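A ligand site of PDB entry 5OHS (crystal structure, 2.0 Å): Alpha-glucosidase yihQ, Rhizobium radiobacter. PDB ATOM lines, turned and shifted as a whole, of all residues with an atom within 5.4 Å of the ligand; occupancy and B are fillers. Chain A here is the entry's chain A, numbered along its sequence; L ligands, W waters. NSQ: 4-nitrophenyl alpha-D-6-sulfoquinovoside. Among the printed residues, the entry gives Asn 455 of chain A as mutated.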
ATOM      1  N   ARG A  42      -5.546 -24.190 -24.712  1.00  0.00           N
ATOM      2  CA  ARG A  42      -6.875 -24.706 -25.048  1.00  0.00           C
ATOM      3  C   ARG A  42      -7.678 -25.228 -23.849  1.00  0.00           C
ATOM      4  O   ARG A  42      -8.256 -26.299 -23.878  1.00  0.00           O
ATOM      5  CB  ARG A  42      -6.721 -25.758 -26.136  1.00  0.00           C
ATOM      6  CG  ARG A  42      -6.040 -25.123 -27.353  1.00  0.00           C
ATOM      7  CD  ARG A  42      -5.773 -26.083 -28.443  1.00  0.00           C
ATOM      8  NE  ARG A  42      -5.208 -25.348 -29.594  1.00  0.00           N
ATOM      9  CZ  ARG A  42      -4.871 -25.921 -30.765  1.00  0.00           C
ATOM     10  NH1 ARG A  42      -5.074 -27.223 -30.935  1.00  0.00           N
ATOM     11  NH2 ARG A  42      -4.459 -25.178 -31.777  1.00  0.00           N
ATOM     12  N   GLU A 135     -10.538 -27.528 -18.374  1.00  0.00           N
ATOM     13  CA  GLU A 135     -10.767 -28.858 -18.931  1.00  0.00           C
ATOM     14  C   GLU A 135     -10.314 -29.919 -17.911  1.00  0.00           C
ATOM     15  O   GLU A 135      -9.259 -29.788 -17.297  1.00  0.00           O
ATOM     16  CB  GLU A 135      -9.981 -29.047 -20.215  1.00  0.00           C
ATOM     17  CG  GLU A 135     -10.487 -28.171 -21.343  1.00  0.00           C
ATOM     18  CD  GLU A 135     -11.933 -28.650 -21.726  1.00  0.00           C
ATOM     19  OE1 GLU A 135     -12.435 -29.921 -21.576  1.00  0.00           O
ATOM     20  OE2 GLU A 135     -12.589 -27.787 -22.190  1.00  0.00           O
ATOM     21  N   LYS A 245     -26.536 -34.636 -34.476  1.00  0.00           N
ATOM     22  CA  LYS A 245     -25.823 -33.530 -35.051  1.00  0.00           C
ATOM     23  C   LYS A 245     -25.577 -33.737 -36.537  1.00  0.00           C
ATOM     24  O   LYS A 245     -24.520 -33.445 -37.062  1.00  0.00           O
ATOM     25  CB  LYS A 245     -24.537 -33.211 -34.307  1.00  0.00           C
ATOM     26  CG  LYS A 245     -23.502 -34.326 -34.095  1.00  0.00           C
ATOM     27  CD  LYS A 245     -22.459 -33.983 -33.090  1.00  0.00           C
ATOM     28  CE  LYS A 245     -21.343 -33.099 -33.613  1.00  0.00           C
ATOM     29  NZ  LYS A 245     -20.371 -32.764 -32.563  1.00  0.00           N
ATOM     30  N   TRP A 268     -32.295 -32.944 -29.373  1.00  0.00           N
ATOM     31  CA  TRP A 268     -31.228 -31.965 -29.052  1.00  0.00           C
ATOM     32  C   TRP A 268     -30.258 -31.975 -30.219  1.00  0.00           C
ATOM     33  O   TRP A 268     -29.573 -32.975 -30.460  1.00  0.00           O
ATOM     34  CB  TRP A 268     -30.557 -32.332 -27.725  1.00  0.00           C
ATOM     35  CG  TRP A 268     -29.283 -31.611 -27.513  1.00  0.00           C
ATOM     36  CD1 TRP A 268     -29.129 -30.261 -27.468  1.00  0.00           C
ATOM     37  CD2 TRP A 268     -28.004 -32.182 -27.317  1.00  0.00           C
ATOM     38  NE1 TRP A 268     -27.800 -29.945 -27.310  1.00  0.00           N
ATOM     39  CE2 TRP A 268     -27.078 -31.103 -27.204  1.00  0.00           C
ATOM     40  CE3 TRP A 268     -27.517 -33.499 -27.219  1.00  0.00           C
ATOM     41  CZ2 TRP A 268     -25.726 -31.305 -27.048  1.00  0.00           C
ATOM     42  CZ3 TRP A 268     -26.147 -33.696 -27.079  1.00  0.00           C
ATOM     43  CH2 TRP A 268     -25.258 -32.608 -26.985  1.00  0.00           C
ATOM     44  N   GLU A 270     -27.189 -29.979 -31.370  1.00  0.00           N
ATOM     45  CA  GLU A 270     -26.166 -28.965 -31.080  1.00  0.00           C
ATOM     46  C   GLU A 270     -25.669 -28.231 -32.329  1.00  0.00           C
ATOM     47  O   GLU A 270     -25.161 -27.091 -32.243  1.00  0.00           O
ATOM     48  CB  GLU A 270     -25.002 -29.540 -30.254  1.00  0.00           C
ATOM     49  CG  GLU A 270     -24.189 -30.645 -30.918  1.00  0.00           C
ATOM     50  CD  GLU A 270     -22.873 -31.005 -30.156  1.00  0.00           C
ATOM     51  OE1 GLU A 270     -22.696 -30.597 -28.997  1.00  0.00           O
ATOM     52  OE2 GLU A 270     -22.051 -31.662 -30.811  1.00  0.00           O
ATOM     53  N   PHE A 280      -9.903 -32.005 -34.438  1.00  0.00           N
ATOM     54  CA  PHE A 280     -10.528 -32.688 -33.312  1.00  0.00           C
ATOM     55  C   PHE A 280     -11.747 -33.482 -33.769  1.00  0.00           C
ATOM     56  O   PHE A 280     -11.989 -34.593 -33.277  1.00  0.00           O
ATOM     57  CB  PHE A 280     -10.909 -31.695 -32.248  1.00  0.00           C
ATOM     58  CG  PHE A 280     -11.439 -32.273 -30.974  1.00  0.00           C
ATOM     59  CD1 PHE A 280     -10.587 -32.776 -30.026  1.00  0.00           C
ATOM     60  CD2 PHE A 280     -12.820 -32.294 -30.739  1.00  0.00           C
ATOM     61  CE1 PHE A 280     -11.070 -33.268 -28.822  1.00  0.00           C
ATOM     62  CE2 PHE A 280     -13.346 -32.809 -29.546  1.00  0.00           C
ATOM     63  CZ  PHE A 280     -12.466 -33.285 -28.560  1.00  0.00           C
ATOM     64  N   ALA A 282     -15.927 -33.060 -35.699  1.00  0.00           N
ATOM     65  CA  ALA A 282     -17.071 -32.274 -36.075  1.00  0.00           C
ATOM     66  C   ALA A 282     -17.481 -31.363 -34.958  1.00  0.00           C
ATOM     67  O   ALA A 282     -18.393 -31.639 -34.193  1.00  0.00           O
ATOM     68  CB  ALA A 282     -18.229 -33.237 -36.458  1.00  0.00           C
ATOM     69  N   ARG A 283     -16.783 -30.235 -34.837  1.00  0.00           N
ATOM     70  CA  ARG A 283     -17.109 -29.236 -33.852  1.00  0.00           C
ATOM     71  C   ARG A 283     -18.199 -28.294 -34.430  1.00  0.00           C
ATOM     72  O   ARG A 283     -18.664 -28.464 -35.561  1.00  0.00           O
ATOM     73  CB  ARG A 283     -15.854 -28.449 -33.469  1.00  0.00           C
ATOM     74  CG  ARG A 283     -14.753 -29.386 -32.879  1.00  0.00           C
ATOM     75  CD  ARG A 283     -13.657 -28.655 -32.175  1.00  0.00           C
ATOM     76  NE  ARG A 283     -14.123 -28.113 -30.901  1.00  0.00           N
ATOM     77  CZ  ARG A 283     -13.409 -27.290 -30.164  1.00  0.00           C
ATOM     78  NH1 ARG A 283     -12.128 -27.007 -30.450  1.00  0.00           N
ATOM     79  NH2 ARG A 283     -13.924 -26.878 -28.996  1.00  0.00           N
ATOM     80  N   LEU A 284     -18.649 -27.364 -33.589  1.00  0.00           N
ATOM     81  CA  LEU A 284     -19.711 -26.472 -33.954  1.00  0.00           C
ATOM     82  C   LEU A 284     -19.210 -25.100 -34.381  1.00  0.00           C
ATOM     83  O   LEU A 284     -18.084 -24.710 -34.075  1.00  0.00           O
ATOM     84  CB  LEU A 284     -20.670 -26.314 -32.772  1.00  0.00           C
ATOM     85  CG  LEU A 284     -21.146 -27.642 -32.164  1.00  0.00           C
ATOM     86  CD1 LEU A 284     -21.994 -27.396 -30.934  1.00  0.00           C
ATOM     87  CD2 LEU A 284     -21.863 -28.549 -33.109  1.00  0.00           C
ATOM     88  N   TRP A 286     -19.443 -21.353 -33.799  1.00  0.00           N
ATOM     89  CA  TRP A 286     -19.799 -20.647 -32.558  1.00  0.00           C
ATOM     90  C   TRP A 286     -20.393 -19.206 -32.825  1.00  0.00           C
ATOM     91  O   TRP A 286     -19.768 -18.145 -32.527  1.00  0.00           O
ATOM     92  CB  TRP A 286     -18.611 -20.586 -31.594  1.00  0.00           C
ATOM     93  CG  TRP A 286     -18.193 -21.917 -31.029  1.00  0.00           C
ATOM     94  CD1 TRP A 286     -18.677 -23.171 -31.358  1.00  0.00           C
ATOM     95  CD2 TRP A 286     -17.207 -22.122 -30.035  1.00  0.00           C
ATOM     96  NE1 TRP A 286     -18.043 -24.140 -30.582  1.00  0.00           N
ATOM     97  CE2 TRP A 286     -17.157 -23.505 -29.754  1.00  0.00           C
ATOM     98  CE3 TRP A 286     -16.418 -21.256 -29.290  1.00  0.00           C
ATOM     99  CZ2 TRP A 286     -16.285 -24.030 -28.792  1.00  0.00           C
ATOM    100  CZ3 TRP A 286     -15.585 -21.773 -28.336  1.00  0.00           C
ATOM    101  CH2 TRP A 286     -15.526 -23.156 -28.094  1.00  0.00           C
ATOM    102  N   TYR A 315     -27.814 -25.383 -28.320  1.00  0.00           N
ATOM    103  CA  TYR A 315     -26.453 -25.279 -27.808  1.00  0.00           C
ATOM    104  C   TYR A 315     -26.044 -23.827 -27.824  1.00  0.00           C
ATOM    105  O   TYR A 315     -26.281 -23.124 -28.807  1.00  0.00           O
ATOM    106  CB  TYR A 315     -25.447 -26.078 -28.719  1.00  0.00           C
ATOM    107  CG  TYR A 315     -24.005 -25.949 -28.259  1.00  0.00           C
ATOM    108  CD1 TYR A 315     -23.263 -24.839 -28.612  1.00  0.00           C
ATOM    109  CD2 TYR A 315     -23.389 -26.922 -27.467  1.00  0.00           C
ATOM    110  CE1 TYR A 315     -21.938 -24.677 -28.169  1.00  0.00           C
ATOM    111  CE2 TYR A 315     -22.056 -26.782 -27.054  1.00  0.00           C
ATOM    112  CZ  TYR A 315     -21.332 -25.656 -27.389  1.00  0.00           C
ATOM    113  OH  TYR A 315     -20.020 -25.471 -26.991  1.00  0.00           O
ATOM    114  N   PHE A 349      -9.319 -21.638 -29.488  1.00  0.00           N
ATOM    115  CA  PHE A 349     -10.077 -22.803 -28.986  1.00  0.00           C
ATOM    116  C   PHE A 349      -9.761 -24.122 -29.669  1.00  0.00           C
ATOM    117  O   PHE A 349     -10.370 -25.134 -29.345  1.00  0.00           O
ATOM    118  CB  PHE A 349     -11.560 -22.524 -29.008  1.00  0.00           C
ATOM    119  CG  PHE A 349     -11.974 -21.622 -27.892  1.00  0.00           C
ATOM    120  CD1 PHE A 349     -11.934 -20.251 -28.048  1.00  0.00           C
ATOM    121  CD2 PHE A 349     -12.423 -22.148 -26.711  1.00  0.00           C
ATOM    122  CE1 PHE A 349     -12.304 -19.414 -27.015  1.00  0.00           C
ATOM    123  CE2 PHE A 349     -12.841 -21.321 -25.689  1.00  0.00           C
ATOM    124  CZ  PHE A 349     -12.755 -19.940 -25.824  1.00  0.00           C
ATOM    125  N   MET A 386     -27.767 -27.174 -24.241  1.00  0.00           N
ATOM    126  CA  MET A 386     -26.505 -27.298 -23.580  1.00  0.00           C
ATOM    127  C   MET A 386     -25.918 -25.892 -23.431  1.00  0.00           C
ATOM    128  O   MET A 386     -25.760 -25.178 -24.432  1.00  0.00           O
ATOM    129  CB  MET A 386     -25.558 -28.188 -24.425  1.00  0.00           C
ATOM    130  CG  MET A 386     -24.139 -28.351 -23.841  1.00  0.00           C
ATOM    131  SD  MET A 386     -23.102 -29.444 -24.811  1.00  0.00           S
ATOM    132  CE  MET A 386     -23.715 -30.999 -24.187  1.00  0.00           C
ATOM    133  N   ASP A 388     -22.696 -24.474 -22.589  1.00  0.00           N
ATOM    134  CA  ASP A 388     -21.389 -25.053 -22.531  1.00  0.00           C
ATOM    135  C   ASP A 388     -20.315 -24.057 -22.106  1.00  0.00           C
ATOM    136  O   ASP A 388     -20.564 -22.856 -22.056  1.00  0.00           O
ATOM    137  CB  ASP A 388     -21.062 -25.643 -23.890  1.00  0.00           C
ATOM    138  CG  ASP A 388     -19.928 -26.691 -23.870  1.00  0.00           C
ATOM    139  OD1 ASP A 388     -19.460 -27.094 -22.766  1.00  0.00           O
ATOM    140  OD2 ASP A 388     -19.502 -27.034 -24.996  1.00  0.00           O
ATOM    141  N   PHE A 389     -19.133 -24.600 -21.779  1.00  0.00           N
ATOM    142  CA  PHE A 389     -17.962 -23.851 -21.406  1.00  0.00           C
ATOM    143  C   PHE A 389     -18.142 -22.998 -20.132  1.00  0.00           C
ATOM    144  O   PHE A 389     -19.038 -23.265 -19.321  1.00  0.00           O
ATOM    145  CB  PHE A 389     -17.397 -23.076 -22.618  1.00  0.00           C
ATOM    146  CG  PHE A 389     -16.736 -23.959 -23.634  1.00  0.00           C
ATOM    147  CD1 PHE A 389     -17.489 -24.585 -24.573  1.00  0.00           C
ATOM    148  CD2 PHE A 389     -15.344 -24.186 -23.602  1.00  0.00           C
ATOM    149  CE1 PHE A 389     -16.892 -25.403 -25.521  1.00  0.00           C
ATOM    150  CE2 PHE A 389     -14.751 -25.004 -24.531  1.00  0.00           C
ATOM    151  CZ  PHE A 389     -15.510 -25.649 -25.482  1.00  0.00           C
ATOM    152  N   TYR A 392     -12.622 -21.446 -19.427  1.00  0.00           N
ATOM    153  CA  TYR A 392     -11.473 -21.021 -20.216  1.00  0.00           C
ATOM    154  C   TYR A 392     -11.031 -19.583 -20.059  1.00  0.00           C
ATOM    155  O   TYR A 392     -10.291 -19.105 -20.935  1.00  0.00           O
ATOM    156  CB  TYR A 392     -11.745 -21.124 -21.701  1.00  0.00           C
ATOM    157  CG  TYR A 392     -11.511 -22.397 -22.372  1.00  0.00           C
ATOM    158  CD1 TYR A 392     -12.200 -23.497 -21.935  1.00  0.00           C
ATOM    159  CD2 TYR A 392     -10.704 -22.510 -23.538  1.00  0.00           C
ATOM    160  CE1 TYR A 392     -12.061 -24.755 -22.557  1.00  0.00           C
ATOM    161  CE2 TYR A 392     -10.576 -23.746 -24.213  1.00  0.00           C
ATOM    162  CZ  TYR A 392     -11.248 -24.872 -23.711  1.00  0.00           C
ATOM    163  OH  TYR A 392     -11.249 -26.166 -24.243  1.00  0.00           O
ATOM    164  N   ARG A 438     -21.713 -28.000 -17.744  1.00  0.00           N
ATOM    165  CA  ARG A 438     -20.635 -28.825 -17.261  1.00  0.00           C
ATOM    166  C   ARG A 438     -19.705 -28.055 -16.349  1.00  0.00           C
ATOM    167  O   ARG A 438     -19.036 -28.701 -15.539  1.00  0.00           O
ATOM    168  CB  ARG A 438     -19.882 -29.490 -18.416  1.00  0.00           C
ATOM    169  CG  ARG A 438     -19.066 -28.549 -19.288  1.00  0.00           C
ATOM    170  CD  ARG A 438     -18.193 -29.400 -20.273  1.00  0.00           C
ATOM    171  NE  ARG A 438     -17.657 -28.524 -21.294  1.00  0.00           N
ATOM    172  CZ  ARG A 438     -16.389 -28.260 -21.563  1.00  0.00           C
ATOM    173  NH1 ARG A 438     -15.405 -28.829 -20.924  1.00  0.00           N
ATOM    174  NH2 ARG A 438     -16.105 -27.391 -22.491  1.00  0.00           N
ATOM    175  N   TRP A 452     -24.433 -31.551 -16.294  1.00  0.00           N
ATOM    176  CA  TRP A 452     -23.957 -32.764 -16.906  1.00  0.00           C
ATOM    177  C   TRP A 452     -22.478 -32.972 -16.627  1.00  0.00           C
ATOM    178  O   TRP A 452     -21.717 -32.010 -16.391  1.00  0.00           O
ATOM    179  CB  TRP A 452     -24.318 -32.892 -18.403  1.00  0.00           C
ATOM    180  CG  TRP A 452     -23.257 -32.615 -19.462  1.00  0.00           C
ATOM    181  CD1 TRP A 452     -22.513 -33.520 -20.150  1.00  0.00           C
ATOM    182  CD2 TRP A 452     -22.920 -31.345 -19.981  1.00  0.00           C
ATOM    183  NE1 TRP A 452     -21.690 -32.896 -21.075  1.00  0.00           N
ATOM    184  CE2 TRP A 452     -21.930 -31.548 -21.001  1.00  0.00           C
ATOM    185  CE3 TRP A 452     -23.410 -30.044 -19.761  1.00  0.00           C
ATOM    186  CZ2 TRP A 452     -21.407 -30.499 -21.756  1.00  0.00           C
ATOM    187  CZ3 TRP A 452     -22.844 -28.972 -20.506  1.00  0.00           C
ATOM    188  CH2 TRP A 452     -21.842 -29.220 -21.473  1.00  0.00           C
ATOM    189  N   GLY A 454     -19.852 -33.476 -18.278  1.00  0.00           N
ATOM    190  CA  GLY A 454     -18.826 -33.084 -19.241  1.00  0.00           C
ATOM    191  C   GLY A 454     -18.431 -34.221 -20.180  1.00  0.00           C
ATOM    192  O   GLY A 454     -19.226 -35.108 -20.454  1.00  0.00           O
ATOM    193  N   ASN A 455     -17.194 -34.162 -20.644  1.00  0.00           N
ATOM    194  CA  ASN A 455     -16.692 -35.144 -21.617  1.00  0.00           C
ATOM    195  C   ASN A 455     -15.981 -36.324 -20.929  1.00  0.00           C
ATOM    196  O   ASN A 455     -14.937 -36.157 -20.389  1.00  0.00           O
ATOM    197  CB  ASN A 455     -15.706 -34.488 -22.596  1.00  0.00           C
ATOM    198  CG  ASN A 455     -16.303 -33.349 -23.371  1.00  0.00           C
ATOM    199  OD1 ASN A 455     -17.509 -33.277 -23.546  1.00  0.00           O
ATOM    200  ND2 ASN A 455     -15.436 -32.428 -23.819  1.00  0.00           N
ATOM    201  N   ASP A 487     -23.568 -37.838 -20.863  1.00  0.00           N
ATOM    202  CA  ASP A 487     -23.726 -38.270 -22.253  1.00  0.00           C
ATOM    203  C   ASP A 487     -23.798 -39.802 -22.292  1.00  0.00           C
ATOM    204  O   ASP A 487     -22.823 -40.481 -21.893  1.00  0.00           O
ATOM    205  CB  ASP A 487     -22.522 -37.869 -23.132  1.00  0.00           C
ATOM    206  CG  ASP A 487     -22.247 -36.390 -23.149  1.00  0.00           C
ATOM    207  OD1 ASP A 487     -23.207 -35.552 -23.182  1.00  0.00           O
ATOM    208  OD2 ASP A 487     -21.034 -36.076 -23.173  1.00  0.00           O
ATOM    209  N   TYR A 491     -18.251 -39.140 -24.719  1.00  0.00           N
ATOM    210  CA  TYR A 491     -18.033 -38.142 -25.733  1.00  0.00           C
ATOM    211  C   TYR A 491     -16.743 -38.335 -26.506  1.00  0.00           C
ATOM    212  O   TYR A 491     -16.769 -38.366 -27.778  1.00  0.00           O
ATOM    213  CB  TYR A 491     -18.045 -36.734 -25.099  1.00  0.00           C
ATOM    214  CG  TYR A 491     -17.718 -35.644 -26.096  1.00  0.00           C
ATOM    215  CD1 TYR A 491     -18.708 -35.087 -26.881  1.00  0.00           C
ATOM    216  CD2 TYR A 491     -16.432 -35.201 -26.266  1.00  0.00           C
ATOM    217  CE1 TYR A 491     -18.424 -34.124 -27.859  1.00  0.00           C
ATOM    218  CE2 TYR A 491     -16.094 -34.268 -27.200  1.00  0.00           C
ATOM    219  CZ  TYR A 491     -17.119 -33.681 -28.013  1.00  0.00           C
ATOM    220  OH  TYR A 491     -16.792 -32.762 -28.971  1.00  0.00           O
ATOM    221  N   HIS A 520     -25.630 -38.373 -27.348  1.00  0.00           N
ATOM    222  CA  HIS A 520     -24.689 -37.404 -27.922  1.00  0.00           C
ATOM    223  C   HIS A 520     -23.931 -38.182 -28.986  1.00  0.00           C
ATOM    224  O   HIS A 520     -23.418 -39.280 -28.693  1.00  0.00           O
ATOM    225  CB  HIS A 520     -23.756 -36.886 -26.859  1.00  0.00           C
ATOM    226  CG  HIS A 520     -23.009 -35.616 -27.187  1.00  0.00           C
ATOM    227  ND1 HIS A 520     -22.664 -35.230 -28.457  1.00  0.00           N
ATOM    228  CD2 HIS A 520     -22.458 -34.663 -26.363  1.00  0.00           C
ATOM    229  CE1 HIS A 520     -21.968 -34.094 -28.408  1.00  0.00           C
ATOM    230  NE2 HIS A 520     -21.853 -33.715 -27.141  1.00  0.00           N
HETATM  231  O12 NSQ L   1     -17.249 -29.367 -30.546  1.00  0.00           O
HETATM  232  S10 NSQ L   1     -17.614 -28.102 -29.865  1.00  0.00           S
HETATM  233  O13 NSQ L   1     -18.040 -27.037 -30.847  1.00  0.00           O
HETATM  234  O11 NSQ L   1     -16.555 -27.435 -29.037  1.00  0.00           O
HETATM  235  C6  NSQ L   1     -18.910 -28.639 -28.969  1.00  0.00           C
HETATM  236  C5  NSQ L   1     -18.556 -29.582 -27.818  1.00  0.00           C
HETATM  237  O5  NSQ L   1     -17.992 -28.716 -26.786  1.00  0.00           O
HETATM  238  C1  NSQ L   1     -17.659 -29.423 -25.585  1.00  0.00           C
HETATM  239  C2  NSQ L   1     -18.891 -30.135 -25.036  1.00  0.00           C
HETATM  240  O2  NSQ L   1     -18.570 -30.753 -23.796  1.00  0.00           O
HETATM  241  C3  NSQ L   1     -19.450 -31.132 -26.017  1.00  0.00           C
HETATM  242  O3  NSQ L   1     -20.623 -31.820 -25.525  1.00  0.00           O
HETATM  243  C4  NSQ L   1     -19.747 -30.374 -27.312  1.00  0.00           C
HETATM  244  O4  NSQ L   1     -20.355 -31.323 -28.231  1.00  0.00           O
HETATM  245  O1  NSQ L   1     -16.656 -30.468 -25.822  1.00  0.00           O
HETATM  246  C25 NSQ L   1     -15.414 -30.066 -26.136  1.00  0.00           C
HETATM  247  C26 NSQ L   1     -14.941 -30.393 -27.385  1.00  0.00           C
HETATM  248  C27 NSQ L   1     -13.644 -30.025 -27.707  1.00  0.00           C
HETATM  249  C28 NSQ L   1     -12.855 -29.357 -26.790  1.00  0.00           C
HETATM  250  N32 NSQ L   1     -11.555 -29.029 -27.163  1.00  0.00           N
HETATM  251  O33 NSQ L   1     -11.156 -29.310 -28.336  1.00  0.00           O
HETATM  252  O34 NSQ L   1     -10.823 -28.484 -26.301  1.00  0.00           O
HETATM  253  C29 NSQ L   1     -13.339 -29.026 -25.533  1.00  0.00           C
HETATM  254  C30 NSQ L   1     -14.631 -29.385 -25.210  1.00  0.00           C
HETATM  255  O   HOH W   1     -12.131 -25.730 -27.060  1.00  0.00           O
HETATM  256  O   HOH W   2      -7.872 -29.032 -25.006  1.00  0.00           O
HETATM  257  O   HOH W   3     -20.213 -33.753 -23.346  1.00  0.00           O
HETATM  258  O   HOH W   4     -18.732 -31.644 -30.459  1.00  0.00           O
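O4 of the ligand lies within hydrogen-bond range of OE1 of Glu 270 (2.6 Å).
O11 of the ligand is in salt-bridge range of NH2 of Arg 283 (2.7 Å).
The side-chain amide oxygen (OD1) of Asn 455 lies within hydrogen-bond range of an oxygen (O2) of the ligand (2.7 Å).
An oxygen (O3) of the ligand lies within hydrogen-bond range of a ring nitrogen (NE2) of His 520, 2.8 Å away.
The backbone NH of Leu 284 sits at hydrogen-bond distance from an oxygen (O13) of the ligand (2.8 Å).
O13 of the ligand sits at hydrogen-bond distance from NE1 of Trp 286, 2.9 Å away.
OH of Tyr 392 sits at hydrogen-bond distance from O34 of the ligand (3.1 Å).
An oxygen (O3) of the ligand sits close to the side-chain sulfur (SD) of Met 386, at 3.5 Å.
An oxygen (O2) of the ligand lies within hydrogen-bond range of the guanidinium group (NE) of Arg 438.
The side-chain amino group (NZ) of Lys 245 lies within salt-bridge range of the side-chain carboxylate (OE2) of Glu 270 (2.7 Å).
The guanidinium group of Arg 283 is in hydrogen-bond range of the backbone carbonyl oxygen of Phe 349, at 2.8 Å.
OD1 of Asp 388 lies within salt-bridge range of NE of Arg 438, at 2.7 Å.
The side-chain carboxylate of Asp 388 lies within hydrogen-bond range of the side-chain hydroxyl of Tyr 315.
The side-chain hydroxyl (OH) of Tyr 392 sits at hydrogen-bond distance from the side-chain carboxylate (OE2) of Glu 135 (2.9 Å).
The side-chain hydroxyl (OH) of Tyr 392 lies within hydrogen-bond range of the backbone carbonyl oxygen (O) of Arg 42.
NH1 of Arg 438 is in salt-bridge range of OE1 of Glu 135 (3.2 Å).
O of Gly 454 lies within hydrogen-bond range of NE1 of Trp 452 (3.4 Å).
An oxygen (O5) of the ligand sits close to the side-chain carboxylate (OD2) of Asp 388, 2.9 Å away.
Residues that only touch the ligand: Glu 135, Phe 280, Tyr 315, Phe 389, Trp 452 and Tyr 491.
16 residues have an atom within 4 Å of the ligand: Glu 135, Glu 270, Phe 280, Arg 283, Leu 284, Trp 286, Tyr 315, Met 386, Asp 388, Phe 389, Tyr 392, Arg 438, Trp 452, Asn 455, Tyr 491 and His 520.
The nearest printed residue that does not touch the ligand is Arg 42 (4.2 Å).
Water W4 lies within hydrogen-bond range of the side-chain hydroxyl of Tyr 491 (2.7 Å), an oxygen (O12) of the ligand (2.7 Å), the side-chain amino group of Lys 245 (2.9 Å) and the side-chain carboxylate of Glu 270 (3.3 Å).
Water W1 lies within hydrogen-bond range of NH2 of Arg 283 (2.9 Å), O of Phe 349 (2.9 Å), OH of Tyr 392 (3.0 Å) and O34 of the ligand (3.1 Å).
Water W2 bridges O of Arg 42 and O34 of the ligand.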
